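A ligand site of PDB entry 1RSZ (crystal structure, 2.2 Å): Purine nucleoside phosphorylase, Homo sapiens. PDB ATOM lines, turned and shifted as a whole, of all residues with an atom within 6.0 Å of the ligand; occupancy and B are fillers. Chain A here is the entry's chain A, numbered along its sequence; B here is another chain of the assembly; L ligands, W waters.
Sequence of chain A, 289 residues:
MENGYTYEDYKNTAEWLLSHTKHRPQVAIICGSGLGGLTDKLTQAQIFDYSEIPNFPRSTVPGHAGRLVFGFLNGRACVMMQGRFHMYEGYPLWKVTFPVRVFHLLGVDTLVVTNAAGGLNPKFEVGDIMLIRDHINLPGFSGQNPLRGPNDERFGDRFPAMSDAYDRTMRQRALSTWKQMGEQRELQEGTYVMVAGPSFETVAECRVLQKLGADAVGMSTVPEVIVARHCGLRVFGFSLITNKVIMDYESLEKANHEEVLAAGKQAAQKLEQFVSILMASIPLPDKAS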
ATOM      1  N   SER A  33      -5.508  -6.066 -16.164  1.00  0.00           N
ATOM      2  CA  SER A  33      -5.540  -4.603 -16.143  1.00  0.00           C
ATOM      3  C   SER A  33      -6.791  -4.057 -16.823  1.00  0.00           C
ATOM      4  O   SER A  33      -7.050  -4.362 -17.991  1.00  0.00           O
ATOM      5  CB  SER A  33      -4.290  -4.058 -16.841  1.00  0.00           C
ATOM      6  OG  SER A  33      -4.384  -2.661 -17.055  1.00  0.00           O
ATOM      7  N   HIS A  86       2.938  -8.271 -10.038  1.00  0.00           N
ATOM      8  CA  HIS A  86       3.793  -8.486 -11.198  1.00  0.00           C
ATOM      9  C   HIS A  86       5.257  -8.550 -10.809  1.00  0.00           C
ATOM     10  O   HIS A  86       5.698  -7.907  -9.859  1.00  0.00           O
ATOM     11  CB  HIS A  86       3.643  -7.355 -12.229  1.00  0.00           C
ATOM     12  CG  HIS A  86       2.237  -7.104 -12.663  1.00  0.00           C
ATOM     13  ND1 HIS A  86       1.370  -6.309 -11.950  1.00  0.00           N
ATOM     14  CD2 HIS A  86       1.545  -7.547 -13.750  1.00  0.00           C
ATOM     15  CE1 HIS A  86       0.207  -6.255 -12.585  1.00  0.00           C
ATOM     16  NE2 HIS A  86       0.288  -6.998 -13.667  1.00  0.00           N
ATOM     17  N   TYR A  88       7.761  -7.328 -12.438  1.00  0.00           N
ATOM     18  CA  TYR A  88       8.400  -6.014 -12.638  1.00  0.00           C
ATOM     19  C   TYR A  88       8.297  -5.065 -11.446  1.00  0.00           C
ATOM     20  O   TYR A  88       9.030  -4.094 -11.371  1.00  0.00           O
ATOM     21  CB  TYR A  88       7.879  -5.332 -13.924  1.00  0.00           C
ATOM     22  CG  TYR A  88       6.394  -4.987 -13.949  1.00  0.00           C
ATOM     23  CD1 TYR A  88       5.847  -4.021 -13.086  1.00  0.00           C
ATOM     24  CD2 TYR A  88       5.528  -5.646 -14.822  1.00  0.00           C
ATOM     25  CE1 TYR A  88       4.486  -3.720 -13.093  1.00  0.00           C
ATOM     26  CE2 TYR A  88       4.165  -5.347 -14.839  1.00  0.00           C
ATOM     27  CZ  TYR A  88       3.647  -4.396 -13.978  1.00  0.00           C
ATOM     28  OH  TYR A  88       2.311  -4.127 -14.004  1.00  0.00           O
ATOM     29  N   ALA A 116      -4.296  -7.889 -20.181  1.00  0.00           N
ATOM     30  CA  ALA A 116      -4.311  -7.007 -21.333  1.00  0.00           C
ATOM     31  C   ALA A 116      -3.007  -7.388 -22.034  1.00  0.00           C
ATOM     32  O   ALA A 116      -2.074  -7.845 -21.377  1.00  0.00           O
ATOM     33  CB  ALA A 116      -4.279  -5.561 -20.896  1.00  0.00           C
ATOM     34  N   ALA A 117      -2.929  -7.226 -23.357  1.00  0.00           N
ATOM     35  CA  ALA A 117      -1.712  -7.596 -24.065  1.00  0.00           C
ATOM     36  C   ALA A 117      -1.537  -6.893 -25.392  1.00  0.00           C
ATOM     37  O   ALA A 117      -2.492  -6.372 -25.974  1.00  0.00           O
ATOM     38  CB  ALA A 117      -1.663  -9.100 -24.278  1.00  0.00           C
ATOM     39  N   GLY A 118      -0.296  -6.879 -25.856  1.00  0.00           N
ATOM     40  CA  GLY A 118       0.010  -6.271 -27.126  1.00  0.00           C
ATOM     41  C   GLY A 118      -0.178  -7.357 -28.170  1.00  0.00           C
ATOM     42  O   GLY A 118       0.078  -8.533 -27.902  1.00  0.00           O
ATOM     43  N   GLY A 119      -0.627  -6.958 -29.354  1.00  0.00           N
ATOM     44  CA  GLY A 119      -0.838  -7.924 -30.406  1.00  0.00           C
ATOM     45  C   GLY A 119       0.421  -8.110 -31.218  1.00  0.00           C
ATOM     46  O   GLY A 119       1.053  -7.148 -31.651  1.00  0.00           O
ATOM     47  N   VAL A 195       6.987 -11.656 -20.886  1.00  0.00           N
ATOM     48  CA  VAL A 195       8.274 -10.963 -20.783  1.00  0.00           C
ATOM     49  C   VAL A 195       8.132 -10.196 -19.478  1.00  0.00           C
ATOM     50  O   VAL A 195       7.025  -9.803 -19.092  1.00  0.00           O
ATOM     51  CB  VAL A 195       8.567  -9.983 -21.945  1.00  0.00           C
ATOM     52  CG1 VAL A 195       8.755 -10.748 -23.238  1.00  0.00           C
ATOM     53  CG2 VAL A 195       7.453  -8.949 -22.059  1.00  0.00           C
ATOM     54  N   SER A 199       9.388  -1.929 -19.079  1.00  0.00           N
ATOM     55  CA  SER A 199       9.428  -1.105 -20.281  1.00  0.00           C
ATOM     56  C   SER A 199       8.812  -1.900 -21.451  1.00  0.00           C
ATOM     57  O   SER A 199       8.785  -3.137 -21.412  1.00  0.00           O
ATOM     58  CB  SER A 199      10.877  -0.680 -20.600  1.00  0.00           C
ATOM     59  OG  SER A 199      11.750  -1.805 -20.716  1.00  0.00           O
ATOM     60  N   PHE A 200       8.302  -1.190 -22.465  1.00  0.00           N
ATOM     61  CA  PHE A 200       7.678  -1.850 -23.607  1.00  0.00           C
ATOM     62  C   PHE A 200       8.727  -2.308 -24.620  1.00  0.00           C
ATOM     63  O   PHE A 200       9.853  -1.781 -24.655  1.00  0.00           O
ATOM     64  CB  PHE A 200       6.653  -0.917 -24.285  1.00  0.00           C
ATOM     65  CG  PHE A 200       5.362  -0.764 -23.534  1.00  0.00           C
ATOM     66  CD1 PHE A 200       4.550  -1.869 -23.271  1.00  0.00           C
ATOM     67  CD2 PHE A 200       4.960   0.484 -23.068  1.00  0.00           C
ATOM     68  CE1 PHE A 200       3.353  -1.734 -22.553  1.00  0.00           C
ATOM     69  CE2 PHE A 200       3.756   0.640 -22.353  1.00  0.00           C
ATOM     70  CZ  PHE A 200       2.956  -0.481 -22.099  1.00  0.00           C
ATOM     71  N   GLU A 201       8.360  -3.273 -25.450  1.00  0.00           N
ATOM     72  CA  GLU A 201       9.285  -3.829 -26.435  1.00  0.00           C
ATOM     73  C   GLU A 201       9.710  -2.870 -27.532  1.00  0.00           C
ATOM     74  O   GLU A 201       8.979  -1.964 -27.916  1.00  0.00           O
ATOM     75  CB  GLU A 201       8.690  -5.065 -27.113  1.00  0.00           C
ATOM     76  CG  GLU A 201       8.233  -6.187 -26.195  1.00  0.00           C
ATOM     77  CD  GLU A 201       7.015  -5.816 -25.364  1.00  0.00           C
ATOM     78  OE1 GLU A 201       6.215  -4.967 -25.817  1.00  0.00           O
ATOM     79  OE2 GLU A 201       6.838  -6.396 -24.266  1.00  0.00           O
ATOM     80  N   VAL A 217       1.661 -10.524 -26.236  1.00  0.00           N
ATOM     81  CA  VAL A 217       2.715 -10.356 -25.242  1.00  0.00           C
ATOM     82  C   VAL A 217       2.254  -9.541 -24.035  1.00  0.00           C
ATOM     83  O   VAL A 217       1.589  -8.524 -24.172  1.00  0.00           O
ATOM     84  CB  VAL A 217       3.938  -9.651 -25.852  1.00  0.00           C
ATOM     85  CG1 VAL A 217       3.544  -8.277 -26.391  1.00  0.00           C
ATOM     86  CG2 VAL A 217       5.034  -9.511 -24.818  1.00  0.00           C
ATOM     87  N   GLY A 218       2.616 -10.029 -22.851  1.00  0.00           N
ATOM     88  CA  GLY A 218       2.282  -9.356 -21.608  1.00  0.00           C
ATOM     89  C   GLY A 218       3.353  -9.669 -20.569  1.00  0.00           C
ATOM     90  O   GLY A 218       4.301 -10.391 -20.855  1.00  0.00           O
ATOM     91  N   MET A 219       3.205  -9.121 -19.366  1.00  0.00           N
ATOM     92  CA  MET A 219       4.184  -9.370 -18.322  1.00  0.00           C
ATOM     93  C   MET A 219       3.612 -10.034 -17.089  1.00  0.00           C
ATOM     94  O   MET A 219       4.041  -9.757 -15.977  1.00  0.00           O
ATOM     95  CB  MET A 219       4.901  -8.069 -17.935  1.00  0.00           C
ATOM     96  CG  MET A 219       4.228  -6.807 -18.426  1.00  0.00           C
ATOM     97  SD  MET A 219       5.365  -5.461 -18.904  1.00  0.00           S
ATOM     98  CE  MET A 219       5.103  -4.317 -17.648  1.00  0.00           C
ATOM     99  N   THR A 242      -4.997  -4.858 -26.330  1.00  0.00           N
ATOM    100  CA  THR A 242      -5.182  -3.434 -26.110  1.00  0.00           C
ATOM    101  C   THR A 242      -4.384  -2.580 -27.077  1.00  0.00           C
ATOM    102  O   THR A 242      -4.512  -1.357 -27.098  1.00  0.00           O
ATOM    103  CB  THR A 242      -4.763  -3.050 -24.686  1.00  0.00           C
ATOM    104  OG1 THR A 242      -3.386  -3.389 -24.498  1.00  0.00           O
ATOM    105  CG2 THR A 242      -5.602  -3.802 -23.668  1.00  0.00           C
ATOM    106  N   ASN A 243      -3.546  -3.221 -27.886  1.00  0.00           N
ATOM    107  CA  ASN A 243      -2.728  -2.475 -28.816  1.00  0.00           C
ATOM    108  C   ASN A 243      -1.937  -3.407 -29.718  1.00  0.00           C
ATOM    109  O   ASN A 243      -1.703  -4.560 -29.368  1.00  0.00           O
ATOM    110  CB  ASN A 243      -1.749  -1.587 -28.046  1.00  0.00           C
ATOM    111  CG  ASN A 243      -0.911  -2.378 -27.043  1.00  0.00           C
ATOM    112  OD1 ASN A 243      -1.441  -2.918 -26.077  1.00  0.00           O
ATOM    113  ND2 ASN A 243       0.383  -2.437 -27.275  1.00  0.00           N
ATOM    114  N   LYS A 244      -1.547  -2.897 -30.870  1.00  0.00           N
ATOM    115  CA  LYS A 244      -0.748  -3.650 -31.817  1.00  0.00           C
ATOM    116  C   LYS A 244       0.681  -3.182 -31.583  1.00  0.00           C
ATOM    117  O   LYS A 244       0.998  -2.010 -31.815  1.00  0.00           O
ATOM    118  CB  LYS A 244      -1.142  -3.340 -33.261  1.00  0.00           C
ATOM    119  CG  LYS A 244      -2.587  -3.613 -33.643  1.00  0.00           C
ATOM    120  CD  LYS A 244      -2.797  -3.259 -35.106  1.00  0.00           C
ATOM    121  CE  LYS A 244      -4.241  -3.375 -35.537  1.00  0.00           C
ATOM    122  NZ  LYS A 244      -4.425  -2.867 -36.942  1.00  0.00           N
ATOM    123  N   VAL A 245       1.543  -4.068 -31.102  1.00  0.00           N
ATOM    124  CA  VAL A 245       2.927  -3.688 -30.833  1.00  0.00           C
ATOM    125  C   VAL A 245       3.548  -3.203 -32.145  1.00  0.00           C
ATOM    126  O   VAL A 245       3.232  -3.721 -33.211  1.00  0.00           O
ATOM    127  CB  VAL A 245       3.719  -4.886 -30.241  1.00  0.00           C
ATOM    128  CG1 VAL A 245       2.969  -5.446 -29.048  1.00  0.00           C
ATOM    129  CG2 VAL A 245       3.918  -5.963 -31.282  1.00  0.00           C
ATOM    130  N   ALA A 255       3.934   2.494 -27.651  1.00  0.00           N
ATOM    131  CA  ALA A 255       3.046   1.762 -26.753  1.00  0.00           C
ATOM    132  C   ALA A 255       3.011   2.553 -25.449  1.00  0.00           C
ATOM    133  O   ALA A 255       4.056   2.963 -24.942  1.00  0.00           O
ATOM    134  CB  ALA A 255       3.590   0.351 -26.511  1.00  0.00           C
ATOM    135  N   ASN A 256       1.820   2.777 -24.915  1.00  0.00           N
ATOM    136  CA  ASN A 256       1.701   3.539 -23.684  1.00  0.00           C
ATOM    137  C   ASN A 256       0.580   3.027 -22.777  1.00  0.00           C
ATOM    138  O   ASN A 256      -0.445   2.537 -23.252  1.00  0.00           O
ATOM    139  CB  ASN A 256       1.492   5.032 -23.989  1.00  0.00           C
ATOM    140  CG  ASN A 256       0.365   5.274 -24.974  1.00  0.00           C
ATOM    141  OD1 ASN A 256      -0.815   5.107 -24.647  1.00  0.00           O
ATOM    142  ND2 ASN A 256       0.719   5.661 -26.201  1.00  0.00           N
ATOM    143  N   HIS A 257       0.796   3.161 -21.477  1.00  0.00           N
ATOM    144  CA  HIS A 257      -0.157   2.720 -20.478  1.00  0.00           C
ATOM    145  C   HIS A 257      -1.504   3.446 -20.639  1.00  0.00           C
ATOM    146  O   HIS A 257      -2.549   2.948 -20.211  1.00  0.00           O
ATOM    147  CB  HIS A 257       0.435   2.994 -19.083  1.00  0.00           C
ATOM    148  CG  HIS A 257      -0.391   2.441 -17.961  1.00  0.00           C
ATOM    149  ND1 HIS A 257      -0.861   1.140 -17.947  1.00  0.00           N
ATOM    150  CD2 HIS A 257      -0.759   2.994 -16.783  1.00  0.00           C
ATOM    151  CE1 HIS A 257      -1.494   0.925 -16.807  1.00  0.00           C
ATOM    152  NE2 HIS A 257      -1.452   2.029 -16.082  1.00  0.00           N
ATOM    153  N   GLU A 258      -1.463   4.605 -21.264  1.00  0.00           N
ATOM    154  CA  GLU A 258      -2.665   5.405 -21.506  1.00  0.00           C
ATOM    155  C   GLU A 258      -3.609   4.595 -22.368  1.00  0.00           C
ATOM    156  O   GLU A 258      -4.734   4.286 -21.962  1.00  0.00           O
ATOM    157  CB  GLU A 258      -2.299   6.693 -22.252  1.00  0.00           C
ATOM    158  CG  GLU A 258      -1.134   7.482 -21.651  1.00  0.00           C
ATOM    159  CD  GLU A 258      -1.437   7.988 -20.259  1.00  0.00           C
ATOM    160  OE1 GLU A 258      -2.449   8.716 -20.096  1.00  0.00           O
ATOM    161  OE2 GLU A 258      -0.677   7.659 -19.317  1.00  0.00           O
ATOM    162  N   VAL A 260      -3.512   1.437 -23.334  1.00  0.00           N
ATOM    163  CA  VAL A 260      -3.874   0.137 -22.771  1.00  0.00           C
ATOM    164  C   VAL A 260      -5.075   0.241 -21.830  1.00  0.00           C
ATOM    165  O   VAL A 260      -6.007  -0.561 -21.902  1.00  0.00           O
ATOM    166  CB  VAL A 260      -2.691  -0.491 -21.981  1.00  0.00           C
ATOM    167  CG1 VAL A 260      -3.105  -1.829 -21.382  1.00  0.00           C
ATOM    168  CG2 VAL A 260      -1.494  -0.656 -22.899  1.00  0.00           C
ATOM    169  N   LEU A 261      -5.060   1.249 -20.958  1.00  0.00           N
ATOM    170  CA  LEU A 261      -6.146   1.470 -20.018  1.00  0.00           C
ATOM    171  C   LEU A 261      -7.421   1.863 -20.748  1.00  0.00           C
ATOM    172  O   LEU A 261      -8.510   1.448 -20.380  1.00  0.00           O
ATOM    173  CB  LEU A 261      -5.763   2.553 -19.016  1.00  0.00           C
ATOM    174  CG  LEU A 261      -4.620   2.213 -18.056  1.00  0.00           C
ATOM    175  CD1 LEU A 261      -4.194   3.465 -17.311  1.00  0.00           C
ATOM    176  CD2 LEU A 261      -5.062   1.123 -17.086  1.00  0.00           C
ATOM    177  N   PHE B 159       5.787   2.460 -17.192  1.00  0.00           N
ATOM    178  CA  PHE B 159       5.935   1.684 -18.425  1.00  0.00           C
ATOM    179  C   PHE B 159       6.493   2.477 -19.618  1.00  0.00           C
ATOM    180  O   PHE B 159       5.804   2.707 -20.605  1.00  0.00           O
ATOM    181  CB  PHE B 159       4.572   1.110 -18.815  1.00  0.00           C
ATOM    182  CG  PHE B 159       3.886   0.357 -17.701  1.00  0.00           C
ATOM    183  CD1 PHE B 159       4.348  -0.878 -17.272  1.00  0.00           C
ATOM    184  CD2 PHE B 159       2.739   0.882 -17.095  1.00  0.00           C
ATOM    185  CE1 PHE B 159       3.683  -1.582 -16.252  1.00  0.00           C
ATOM    186  CE2 PHE B 159       2.073   0.191 -16.078  1.00  0.00           C
ATOM    187  CZ  PHE B 159       2.548  -1.045 -15.661  1.00  0.00           C
HETATM  188  O1  LIG L   1      -0.055  -0.728 -19.801  1.00  0.00           O
HETATM  189  C1  LIG L   1       0.753  -1.724 -19.208  1.00  0.00           C
HETATM  190  C2  LIG L   1       0.323  -2.977 -18.539  1.00  0.00           C
HETATM  191  C3  LIG L   1      -0.430  -3.809 -19.503  1.00  0.00           C
HETATM  192  C4  LIG L   1       1.462  -3.796 -18.036  1.00  0.00           C
HETATM  193  O2  LIG L   1       1.336  -4.350 -16.725  1.00  0.00           O
HETATM  194  C5  LIG L   1       1.554  -4.685 -19.217  1.00  0.00           C
HETATM  195  N1  LIG L   1       0.220  -5.101 -19.570  1.00  0.00           N
HETATM  196  C6  LIG L   1       0.056  -5.710 -20.873  1.00  0.00           C
HETATM  197  C7  LIG L   1       0.402  -5.147 -22.203  1.00  0.00           C
HETATM  198  C8  LIG L   1      -0.378  -4.410 -23.073  1.00  0.00           C
HETATM  199  N2  LIG L   1       0.221  -4.045 -24.172  1.00  0.00           N
HETATM  200  C9  LIG L   1       1.502  -4.553 -24.072  1.00  0.00           C
HETATM  201  C10 LIG L   1       2.637  -4.454 -24.997  1.00  0.00           C
HETATM  202  O3  LIG L   1       2.652  -3.881 -26.076  1.00  0.00           O
HETATM  203  N3  LIG L   1       3.820  -5.115 -24.541  1.00  0.00           N
HETATM  204  C11 LIG L   1       3.916  -5.814 -23.303  1.00  0.00           C
HETATM  205  N4  LIG L   1       2.851  -5.900 -22.433  1.00  0.00           N
HETATM  206  C12 LIG L   1       1.658  -5.249 -22.865  1.00  0.00           C
HETATM  207  O   HOH W   1       4.932  -2.896 -27.241  1.00  0.00           O
HETATM  208  O   HOH W   2       1.261  -7.438 -17.488  1.00  0.00           O
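OD1 of Asn 243 sits at hydrogen-bond distance from OG1 of Thr 242, 2.5 Å away.
N of Gly 119 is in hydrogen-bond range of O of Asn 243, at 2.6 Å.
ND1 of His 86 sits at hydrogen-bond distance from OH of Tyr 88 (3.1 Å).
The backbone NH (N) of Gly 118 is in hydrogen-bond range of the backbone carbonyl oxygen (O) of Val 217 (3.0 Å).
The backbone carbonyl oxygen of Gly 119 sits close to the backbone NH of Val 245.
O of Ala 117 is in hydrogen-bond range of N of Thr 242, at 2.9 Å.
The backbone NH (N) of Val 195 sits at hydrogen-bond distance from the backbone carbonyl oxygen (O) of Gly 218, at 3.0 Å.
Water W1 lies within hydrogen-bond range of an oxygen (O3) of the ligand (2.7 Å) and the side-chain carboxylate (OE1) of Glu 201 (2.8 Å).
Water W2 bridges an oxygen (O2) of the ligand (3.2 Å) and the backbone NH (N) of Met 219 (3.2 Å).
Ala 116 touches the ligand.
Ala 117 touches the ligand (C to N2, 3.6 Å).
CD1 of Phe 200 touches N3 of the ligand (3.6 Å).
Gly 218 touches the ligand (CA to N4, 3.6 Å).
CG of Met 219 touches C5 of the ligand, 3.5 Å away.
OG1 of Thr 242 touches C8 of the ligand, 3.5 Å away.
CG1 of Val 245 touches O3 of the ligand (3.4 Å).
CG2 of Val 260 touches O1 of the ligand, 3.4 Å away.
Phe 159 of chain B touches the ligand.
15 residues have an atom within 4 Å of the ligand: Tyr 88, Ala 116, Ala 117, Gly 118, Phe 200, Glu 201, Val 217, Gly 218, Met 219, Thr 242, Asn 243, Val 245, His 257, Val 260 and Phe 159 of chain B.
The side-chain carboxylate of Glu 201 is in hydrogen-bond range of a nitrogen (N3) of the ligand (2.7 Å).
A ring nitrogen (ND1) of His 257 lies within hydrogen-bond range of an oxygen (O1) of the ligand (2.8 Å).
OD1 of Asn 243 lies within hydrogen-bond range of N2 of the ligand (2.8 Å).
An oxygen (O2) of the ligand lies within hydrogen-bond range of the side-chain hydroxyl of Tyr 88 (2.9 Å).
N2 of the ligand lies close to N of Gly 118, at 3.3 Å.
The backbone carbonyl oxygen of Val 217 sits close to a nitrogen (N4) of the ligand (3.4 Å).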
